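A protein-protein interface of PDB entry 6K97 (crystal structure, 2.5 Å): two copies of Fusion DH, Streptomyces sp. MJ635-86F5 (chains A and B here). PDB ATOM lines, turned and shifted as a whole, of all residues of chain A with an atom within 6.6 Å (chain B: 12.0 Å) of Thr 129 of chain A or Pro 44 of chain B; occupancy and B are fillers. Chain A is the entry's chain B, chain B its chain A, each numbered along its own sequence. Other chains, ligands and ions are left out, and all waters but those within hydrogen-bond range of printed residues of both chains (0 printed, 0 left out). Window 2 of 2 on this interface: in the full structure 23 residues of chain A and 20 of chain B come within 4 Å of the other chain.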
ATOM      1  N   LEU A  49     -25.695  -7.879  18.537  1.00  0.00           N
ATOM      2  CA  LEU A  49     -25.441  -9.131  19.205  1.00  0.00           C
ATOM      3  C   LEU A  49     -24.468  -8.843  20.355  1.00  0.00           C
ATOM      4  O   LEU A  49     -23.442  -8.192  20.154  1.00  0.00           O
ATOM      5  CB  LEU A  49     -24.795 -10.150  18.267  1.00  0.00           C
ATOM      6  CG  LEU A  49     -24.407 -11.493  18.928  1.00  0.00           C
ATOM      7  CD1 LEU A  49     -25.624 -12.332  19.296  1.00  0.00           C
ATOM      8  CD2 LEU A  49     -23.463 -12.326  18.056  1.00  0.00           C
ATOM      9  N   GLN A 114     -25.981 -15.039  25.318  1.00  0.00           N
ATOM     10  CA  GLN A 114     -26.206 -14.253  24.135  1.00  0.00           C
ATOM     11  C   GLN A 114     -27.465 -13.372  24.232  1.00  0.00           C
ATOM     12  O   GLN A 114     -28.508 -13.821  24.680  1.00  0.00           O
ATOM     13  CB  GLN A 114     -26.318 -15.321  23.069  1.00  0.00           C
ATOM     14  CG  GLN A 114     -26.321 -14.930  21.642  1.00  0.00           C
ATOM     15  CD  GLN A 114     -25.731 -16.043  20.800  1.00  0.00           C
ATOM     16  OE1 GLN A 114     -26.432 -16.622  19.947  1.00  0.00           O
ATOM     17  NE2 GLN A 114     -24.424 -16.344  21.017  1.00  0.00           N
ATOM     18  N   VAL A 115     -27.319 -12.077  23.908  1.00  0.00           N
ATOM     19  CA  VAL A 115     -28.439 -11.157  23.795  1.00  0.00           C
ATOM     20  C   VAL A 115     -28.528 -10.674  22.348  1.00  0.00           C
ATOM     21  O   VAL A 115     -27.554 -10.152  21.831  1.00  0.00           O
ATOM     22  CB  VAL A 115     -28.249  -9.912  24.685  1.00  0.00           C
ATOM     23  CG1 VAL A 115     -29.462  -9.013  24.574  1.00  0.00           C
ATOM     24  CG2 VAL A 115     -28.005 -10.295  26.145  1.00  0.00           C
ATOM     25  N   ALA A 116     -29.680 -10.853  21.709  1.00  0.00           N
ATOM     26  CA  ALA A 116     -29.877 -10.400  20.329  1.00  0.00           C
ATOM     27  C   ALA A 116     -30.925  -9.311  20.272  1.00  0.00           C
ATOM     28  O   ALA A 116     -32.008  -9.433  20.878  1.00  0.00           O
ATOM     29  CB  ALA A 116     -30.307 -11.540  19.432  1.00  0.00           C
ATOM     30  N   VAL A 117     -30.597  -8.243  19.554  1.00  0.00           N
ATOM     31  CA  VAL A 117     -31.526  -7.145  19.354  1.00  0.00           C
ATOM     32  C   VAL A 117     -31.810  -6.921  17.872  1.00  0.00           C
ATOM     33  O   VAL A 117     -30.892  -6.749  17.060  1.00  0.00           O
ATOM     34  CB  VAL A 117     -30.922  -5.875  19.931  1.00  0.00           C
ATOM     35  CG1 VAL A 117     -31.814  -4.710  19.659  1.00  0.00           C
ATOM     36  CG2 VAL A 117     -30.698  -6.077  21.414  1.00  0.00           C
ATOM     37  N   GLY A 118     -33.093  -6.891  17.528  1.00  0.00           N
ATOM     38  CA  GLY A 118     -33.514  -6.611  16.155  1.00  0.00           C
ATOM     39  C   GLY A 118     -33.305  -5.162  15.766  1.00  0.00           C
ATOM     40  O   GLY A 118     -32.928  -4.331  16.604  1.00  0.00           O
ATOM     41  N   SER A 127     -37.023  -5.775  18.833  1.00  0.00           N
ATOM     42  CA  SER A 127     -37.202  -7.013  19.559  1.00  0.00           C
ATOM     43  C   SER A 127     -35.933  -7.282  20.352  1.00  0.00           C
ATOM     44  O   SER A 127     -34.848  -6.801  20.005  1.00  0.00           O
ATOM     45  CB  SER A 127     -37.407  -8.149  18.597  1.00  0.00           C
ATOM     46  OG  SER A 127     -36.138  -8.426  18.014  1.00  0.00           O
ATOM     47  N   LEU A 128     -36.070  -8.068  21.408  1.00  0.00           N
ATOM     48  CA  LEU A 128     -34.917  -8.465  22.207  1.00  0.00           C
ATOM     49  C   LEU A 128     -35.103  -9.918  22.619  1.00  0.00           C
ATOM     50  O   LEU A 128     -36.209 -10.282  22.976  1.00  0.00           O
ATOM     51  CB  LEU A 128     -34.802  -7.553  23.437  1.00  0.00           C
ATOM     52  CG  LEU A 128     -33.634  -7.890  24.368  1.00  0.00           C
ATOM     53  CD1 LEU A 128     -33.017  -6.626  24.936  1.00  0.00           C
ATOM     54  CD2 LEU A 128     -34.062  -8.795  25.493  1.00  0.00           C
ATOM     55  N   THR A 129     -34.042 -10.727  22.547  1.00  0.00           N
ATOM     56  CA  THR A 129     -34.066 -12.121  23.044  1.00  0.00           C
ATOM     57  C   THR A 129     -32.770 -12.455  23.803  1.00  0.00           C
ATOM     58  O   THR A 129     -31.697 -11.972  23.465  1.00  0.00           O
ATOM     59  CB  THR A 129     -34.377 -13.193  21.946  1.00  0.00           C
ATOM     60  OG1 THR A 129     -33.348 -13.229  20.967  1.00  0.00           O
ATOM     61  CG2 THR A 129     -35.645 -12.824  21.208  1.00  0.00           C
ATOM     62  N   ILE A 130     -32.895 -13.267  24.851  1.00  0.00           N
ATOM     63  CA  ILE A 130     -31.760 -13.735  25.624  1.00  0.00           C
ATOM     64  C   ILE A 130     -31.811 -15.254  25.661  1.00  0.00           C
ATOM     65  O   ILE A 130     -32.840 -15.862  25.980  1.00  0.00           O
ATOM     66  CB  ILE A 130     -31.770 -13.180  27.061  1.00  0.00           C
ATOM     67  CG1 ILE A 130     -31.884 -11.646  27.055  1.00  0.00           C
ATOM     68  CG2 ILE A 130     -30.493 -13.587  27.787  1.00  0.00           C
ATOM     69  CD1 ILE A 130     -32.048 -11.006  28.436  1.00  0.00           C
ATOM     70  N   ARG A 131     -30.666 -15.859  25.370  1.00  0.00           N
ATOM     71  CA  ARG A 131     -30.563 -17.288  25.257  1.00  0.00           C
ATOM     72  C   ARG A 131     -29.191 -17.779  25.663  1.00  0.00           C
ATOM     73  O   ARG A 131     -28.234 -16.991  25.706  1.00  0.00           O
ATOM     74  CB  ARG A 131     -30.837 -17.679  23.834  1.00  0.00           C
ATOM     75  CG  ARG A 131     -29.769 -17.227  22.897  1.00  0.00           C
ATOM     76  CD  ARG A 131     -30.193 -17.681  21.526  1.00  0.00           C
ATOM     77  NE  ARG A 131     -29.089 -17.458  20.609  1.00  0.00           N
ATOM     78  CZ  ARG A 131     -28.994 -17.990  19.396  1.00  0.00           C
ATOM     79  NH1 ARG A 131     -27.937 -17.681  18.670  1.00  0.00           N
ATOM     80  NH2 ARG A 131     -29.950 -18.793  18.908  1.00  0.00           N
ATOM     81  N   GLU A 142     -33.946 -20.481  25.236  1.00  0.00           N
ATOM     82  CA  GLU A 142     -34.402 -19.117  25.333  1.00  0.00           C
ATOM     83  C   GLU A 142     -34.844 -18.880  26.782  1.00  0.00           C
ATOM     84  O   GLU A 142     -35.714 -19.597  27.314  1.00  0.00           O
ATOM     85  CB  GLU A 142     -35.558 -18.851  24.375  1.00  0.00           C
ATOM     86  CG  GLU A 142     -36.028 -17.379  24.446  1.00  0.00           C
ATOM     87  CD  GLU A 142     -37.071 -16.989  23.411  1.00  0.00           C
ATOM     88  OE1 GLU A 142     -36.728 -16.926  22.196  1.00  0.00           O
ATOM     89  OE2 GLU A 142     -38.233 -16.724  23.810  1.00  0.00           O
ATOM     90  N   ALA A 144     -35.405 -15.409  27.898  1.00  0.00           N
ATOM     91  CA  ALA A 144     -36.188 -14.189  27.927  1.00  0.00           C
ATOM     92  C   ALA A 144     -36.377 -13.600  26.528  1.00  0.00           C
ATOM     93  O   ALA A 144     -35.510 -13.728  25.664  1.00  0.00           O
ATOM     94  CB  ALA A 144     -35.532 -13.140  28.828  1.00  0.00           C
ATOM     95  N   ASP A 145     -37.505 -12.936  26.346  1.00  0.00           N
ATOM     96  CA  ASP A 145     -37.646 -12.072  25.208  1.00  0.00           C
ATOM     97  C   ASP A 145     -38.564 -10.922  25.548  1.00  0.00           C
ATOM     98  O   ASP A 145     -39.162 -10.876  26.615  1.00  0.00           O
ATOM     99  CB  ASP A 145     -38.140 -12.854  23.990  1.00  0.00           C
ATOM    100  CG  ASP A 145     -39.567 -13.356  24.166  1.00  0.00           C
ATOM    101  OD1 ASP A 145     -39.863 -14.537  23.964  1.00  0.00           O
ATOM    102  OD2 ASP A 145     -40.422 -12.567  24.569  1.00  0.00           O
ATOM    103  N   GLY A 146     -38.633  -9.968  24.636  1.00  0.00           N
ATOM    104  CA  GLY A 146     -39.400  -8.761  24.854  1.00  0.00           C
ATOM    105  C   GLY A 146     -39.072  -7.729  23.817  1.00  0.00           C
ATOM    106  O   GLY A 146     -38.676  -8.076  22.689  1.00  0.00           O
ATOM    107  N   GLY B  28     -18.059 -16.143  24.981  1.00  0.00           N
ATOM    108  CA  GLY B  28     -19.446 -16.509  24.780  1.00  0.00           C
ATOM    109  C   GLY B  28     -19.763 -16.945  23.371  1.00  0.00           C
ATOM    110  O   GLY B  28     -20.920 -16.988  23.039  1.00  0.00           O
ATOM    111  N   LEU B  29     -18.762 -17.232  22.532  1.00  0.00           N
ATOM    112  CA  LEU B  29     -18.981 -17.650  21.113  1.00  0.00           C
ATOM    113  C   LEU B  29     -18.548 -19.064  20.776  1.00  0.00           C
ATOM    114  O   LEU B  29     -17.726 -19.640  21.438  1.00  0.00           O
ATOM    115  CB  LEU B  29     -18.213 -16.728  20.168  1.00  0.00           C
ATOM    116  CG  LEU B  29     -18.671 -15.280  20.264  1.00  0.00           C
ATOM    117  CD1 LEU B  29     -17.484 -14.357  20.570  1.00  0.00           C
ATOM    118  CD2 LEU B  29     -19.394 -14.835  18.996  1.00  0.00           C
ATOM    119  N   GLU B  30     -19.070 -19.577  19.682  1.00  0.00           N
ATOM    120  CA  GLU B  30     -18.722 -20.894  19.164  1.00  0.00           C
ATOM    121  C   GLU B  30     -17.609 -20.713  18.147  1.00  0.00           C
ATOM    122  O   GLU B  30     -17.685 -19.823  17.295  1.00  0.00           O
ATOM    123  CB  GLU B  30     -19.969 -21.573  18.532  1.00  0.00           C
ATOM    124  CG  GLU B  30     -21.073 -21.860  19.553  1.00  0.00           C
ATOM    125  CD  GLU B  30     -22.524 -21.671  19.070  1.00  0.00           C
ATOM    126  OE1 GLU B  30     -22.877 -20.689  18.353  1.00  0.00           O
ATOM    127  OE2 GLU B  30     -23.351 -22.519  19.452  1.00  0.00           O
ATOM    128  N   ALA B  40     -18.167 -18.743  14.663  1.00  0.00           N
ATOM    129  CA  ALA B  40     -19.424 -18.913  13.894  1.00  0.00           C
ATOM    130  C   ALA B  40     -20.593 -18.980  14.826  1.00  0.00           C
ATOM    131  O   ALA B  40     -20.560 -19.757  15.726  1.00  0.00           O
ATOM    132  CB  ALA B  40     -19.371 -20.207  13.123  1.00  0.00           C
ATOM    133  N   THR B  41     -21.633 -18.178  14.660  1.00  0.00           N
ATOM    134  CA  THR B  41     -22.753 -18.316  15.532  1.00  0.00           C
ATOM    135  C   THR B  41     -24.026 -18.188  14.773  1.00  0.00           C
ATOM    136  O   THR B  41     -24.110 -17.399  13.843  1.00  0.00           O
ATOM    137  CB  THR B  41     -22.736 -17.296  16.689  1.00  0.00           C
ATOM    138  OG1 THR B  41     -23.582 -16.200  16.373  1.00  0.00           O
ATOM    139  CG2 THR B  41     -21.375 -16.745  16.960  1.00  0.00           C
ATOM    140  N   GLU B  42     -25.032 -18.964  15.155  1.00  0.00           N
ATOM    141  CA  GLU B  42     -26.336 -18.908  14.520  1.00  0.00           C
ATOM    142  C   GLU B  42     -27.070 -17.948  15.384  1.00  0.00           C
ATOM    143  O   GLU B  42     -26.919 -18.012  16.592  1.00  0.00           O
ATOM    144  CB  GLU B  42     -27.033 -20.285  14.490  1.00  0.00           C
ATOM    145  CG  GLU B  42     -28.339 -20.302  13.664  1.00  0.00           C
ATOM    146  CD  GLU B  42     -29.130 -21.627  13.755  1.00  0.00           C
ATOM    147  OE1 GLU B  42     -29.561 -21.951  14.885  1.00  0.00           O
ATOM    148  OE2 GLU B  42     -29.369 -22.310  12.728  1.00  0.00           O
ATOM    149  N   LEU B  43     -27.795 -17.009  14.786  1.00  0.00           N
ATOM    150  CA  LEU B  43     -28.470 -15.974  15.557  1.00  0.00           C
ATOM    151  C   LEU B  43     -29.905 -16.401  15.666  1.00  0.00           C
ATOM    152  O   LEU B  43     -30.378 -17.174  14.850  1.00  0.00           O
ATOM    153  CB  LEU B  43     -28.360 -14.641  14.856  1.00  0.00           C
ATOM    154  CG  LEU B  43     -26.929 -14.222  14.505  1.00  0.00           C
ATOM    155  CD1 LEU B  43     -26.938 -13.155  13.432  1.00  0.00           C
ATOM    156  CD2 LEU B  43     -26.232 -13.718  15.750  1.00  0.00           C
ATOM    157  N   PRO B  44     -30.626 -15.907  16.665  1.00  0.00           N
ATOM    158  CA  PRO B  44     -32.003 -16.345  16.838  1.00  0.00           C
ATOM    159  C   PRO B  44     -32.897 -16.255  15.594  1.00  0.00           C
ATOM    160  O   PRO B  44     -33.811 -17.059  15.428  1.00  0.00           O
ATOM    161  CB  PRO B  44     -32.525 -15.421  17.931  1.00  0.00           C
ATOM    162  CG  PRO B  44     -31.296 -15.026  18.690  1.00  0.00           C
ATOM    163  CD  PRO B  44     -30.262 -14.849  17.610  1.00  0.00           C
ATOM    164  N   ASP B  45     -32.625 -15.314  14.703  1.00  0.00           N
ATOM    165  CA  ASP B  45     -33.490 -15.154  13.545  1.00  0.00           C
ATOM    166  C   ASP B  45     -33.173 -16.168  12.412  1.00  0.00           C
ATOM    167  O   ASP B  45     -33.852 -16.157  11.389  1.00  0.00           O
ATOM    168  CB  ASP B  45     -33.516 -13.675  13.095  1.00  0.00           C
ATOM    169  CG  ASP B  45     -32.205 -13.205  12.423  1.00  0.00           C
ATOM    170  OD1 ASP B  45     -31.141 -13.914  12.447  1.00  0.00           O
ATOM    171  OD2 ASP B  45     -32.270 -12.094  11.807  1.00  0.00           O
ATOM    172  N   GLY B  46     -32.193 -17.064  12.639  1.00  0.00           N
ATOM    173  CA  GLY B  46     -31.763 -18.092  11.673  1.00  0.00           C
ATOM    174  C   GLY B  46     -30.573 -17.664  10.805  1.00  0.00           C
ATOM    175  O   GLY B  46     -30.128 -18.394   9.908  1.00  0.00           O
ATOM    176  N   GLY B  47     -30.071 -16.454  11.046  1.00  0.00           N
ATOM    177  CA  GLY B  47     -28.917 -15.918  10.324  1.00  0.00           C
ATOM    178  C   GLY B  47     -27.654 -16.374  10.982  1.00  0.00           C
ATOM    179  O   GLY B  47     -27.720 -17.035  12.011  1.00  0.00           O
ATOM    180  N   TYR B  48     -26.508 -16.062  10.379  1.00  0.00           N
ATOM    181  CA  TYR B  48     -25.213 -16.435  10.981  1.00  0.00           C
ATOM    182  C   TYR B  48     -24.242 -15.243  11.042  1.00  0.00           C
ATOM    183  O   TYR B  48     -24.365 -14.301  10.249  1.00  0.00           O
ATOM    184  CB  TYR B  48     -24.565 -17.543  10.180  1.00  0.00           C
ATOM    185  CG  TYR B  48     -25.224 -18.866  10.263  1.00  0.00           C
ATOM    186  CD1 TYR B  48     -26.300 -19.186   9.449  1.00  0.00           C
ATOM    187  CD2 TYR B  48     -24.776 -19.834  11.171  1.00  0.00           C
ATOM    188  CE1 TYR B  48     -26.921 -20.431   9.547  1.00  0.00           C
ATOM    189  CE2 TYR B  48     -25.383 -21.089  11.261  1.00  0.00           C
ATOM    190  CZ  TYR B  48     -26.452 -21.380  10.458  1.00  0.00           C
ATOM    191  OH  TYR B  48     -27.047 -22.625  10.539  1.00  0.00           O
ATOM    192  N   LEU B  49     -23.290 -15.280  11.973  1.00  0.00           N
ATOM    193  CA  LEU B  49     -22.194 -14.294  12.035  1.00  0.00           C
ATOM    194  C   LEU B  49     -20.881 -15.072  12.101  1.00  0.00           C
ATOM    195  O   LEU B  49     -20.760 -15.986  12.914  1.00  0.00           O
ATOM    196  CB  LEU B  49     -22.315 -13.392  13.263  1.00  0.00           C
ATOM    197  CG  LEU B  49     -21.156 -12.388  13.437  1.00  0.00           C
ATOM    198  CD1 LEU B  49     -21.195 -11.278  12.376  1.00  0.00           C
ATOM    199  CD2 LEU B  49     -21.113 -11.742  14.813  1.00  0.00           C
ATOM    200  N   VAL B 117     -24.628 -13.521   7.473  1.00  0.00           N
ATOM    201  CA  VAL B 117     -25.627 -14.170   6.668  1.00  0.00           C
ATOM    202  C   VAL B 117     -27.056 -13.991   7.223  1.00  0.00           C
ATOM    203  O   VAL B 117     -27.341 -14.271   8.402  1.00  0.00           O
ATOM    204  CB  VAL B 117     -25.296 -15.631   6.614  1.00  0.00           C
ATOM    205  CG1 VAL B 117     -26.330 -16.395   5.812  1.00  0.00           C
ATOM    206  CG2 VAL B 117     -23.919 -15.794   6.016  1.00  0.00           C
ATOM    207  N   GLY B 118     -27.962 -13.567   6.369  1.00  0.00           N
ATOM    208  CA  GLY B 118     -29.360 -13.434   6.731  1.00  0.00           C
ATOM    209  C   GLY B 118     -30.050 -14.779   6.857  1.00  0.00           C
ATOM    210  O   GLY B 118     -29.461 -15.839   6.548  1.00  0.00           O
ATOM    211  N   PRO B 119     -31.311 -14.747   7.325  1.00  0.00           N
ATOM    212  CA  PRO B 119     -32.186 -15.926   7.369  1.00  0.00           C
ATOM    213  C   PRO B 119     -32.598 -16.370   5.992  1.00  0.00           C
ATOM    214  O   PRO B 119     -32.523 -15.590   5.061  1.00  0.00           O
ATOM    215  CB  PRO B 119     -33.447 -15.424   8.109  1.00  0.00           C
ATOM    216  CG  PRO B 119     -33.217 -13.967   8.417  1.00  0.00           C
ATOM    217  CD  PRO B 119     -32.024 -13.491   7.668  1.00  0.00           C
ATOM    218  N   ALA B 120     -33.058 -17.609   5.875  1.00  0.00           N
ATOM    219  CA  ALA B 120     -33.495 -18.173   4.613  1.00  0.00           C
ATOM    220  C   ALA B 120     -34.860 -17.658   4.189  1.00  0.00           C
ATOM    221  O   ALA B 120     -35.743 -17.592   5.001  1.00  0.00           O
ATOM    222  CB  ALA B 120     -33.531 -19.698   4.697  1.00  0.00           C
ATOM    223  N   ARG B 126     -30.281 -16.771   1.000  1.00  0.00           N
ATOM    224  CA  ARG B 126     -29.885 -15.908   2.101  1.00  0.00           C
ATOM    225  C   ARG B 126     -29.026 -14.757   1.595  1.00  0.00           C
ATOM    226  O   ARG B 126     -28.185 -14.961   0.779  1.00  0.00           O
ATOM    227  CB  ARG B 126     -29.072 -16.704   3.094  1.00  0.00           C
ATOM    228  CG  ARG B 126     -29.810 -17.875   3.749  1.00  0.00           C
ATOM    229  CD  ARG B 126     -28.792 -18.765   4.451  1.00  0.00           C
ATOM    230  NE  ARG B 126     -29.365 -19.889   5.183  1.00  0.00           N
ATOM    231  CZ  ARG B 126     -29.731 -19.844   6.453  1.00  0.00           C
ATOM    232  NH1 ARG B 126     -29.590 -18.740   7.175  1.00  0.00           N
ATOM    233  NH2 ARG B 126     -30.190 -20.902   7.014  1.00  0.00           N
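Leu 43 of chain B touches Leu 49 of chain A. Glu 42 of chain B touches Gln 114 of chain A. Ala 116 of chain A touches Pro 44 of chain B. Thr 129 of chain A touches Pro 44 of chain B (OG1 to CG, 3.6 Å). CA of Leu 43 of chain B touches NH1 of Arg 131 of chain A, at 3.6 Å. Pro 44 of chain B touches Arg 131 of chain A.
Positions printed for both chains: 49, 117 and 118. Of the 7 pairs that touch across the chains among the printed residues, none has its exchanged pair printed and touching as well.
Of the 18 printed residues of chain B, 3 touch a printed residue of chain A. Hydrophobic or aromatic side chains of chain B within 4 Å of the printed part of chain A: Leu 43 and Pro 44. Along chain B the printed residues that touch a printed residue of chain A span positions 42 to 44. Of the 15 printed residues of chain A, 5 touch a printed residue of chain B. Among the printed residues, 7 pairs touch across the chains. Among the printed residues, no Asp or Glu carboxylate lies within 4 Å of a Lys or Arg side-chain nitrogen of the other chain.
Printed residues of chain B within 4 Å of Leu 49 of chain A: Leu 43. Printed residues of chain B within 4 Å of Gln 114 of chain A: Glu 42 (3.7 Å). No residue of chain B comes within 4 Å of Ser 127 of chain A. Leu 128 of chain A touches none of the printed residues of chain B. Ile 130 of chain A touches none of the printed residues of chain B. Arg 131 of chain A touches just these residues of chain B: Glu 42 (2.3 Å), Leu 43 (3.6 Å) and Pro 44 (3.7 Å). No residue of chain B comes within 4 Å of Asp 145 of chain A. No residue of chain B comes within 4 Å of Gly 146 of chain A. Of the printed residues of chain A, Glu 42 of chain B touches Gln 114 and Arg 131. Of the printed residues of chain A, Leu 43 of chain B touches Leu 49 and Arg 131. Of chain A, only Ala 116, Thr 129 and Arg 131 come within 4 Å of Pro 44 of chain B. The nearest residue of chain B that does not touch Thr 129 of chain A is Asp 45 of chain B (6.6 Å). The nearest printed residue of chain A that does not touch Glu 42 of chain B is Leu 49 of chain A (6.4 Å).
The side-chain carboxylate (OE2) of Glu 42 of chain B sits at hydrogen-bond distance from the side-chain hydroxyl (OH) of Tyr 48 of chain B. The backbone NH (N) of Ala 116 of chain A lies within hydrogen-bond range of the backbone carbonyl oxygen (O) of Thr 129 of chain A, at 2.9 Å. OE1 of Gln 114 of chain A sits at hydrogen-bond distance from NE of Arg 131 of chain A (2.9 Å).
The backbone carbonyl oxygen (O) of Glu 42 of chain B lies close to the guanidinium group (NH1) of Arg 131 of chain A, 2.3 Å away.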
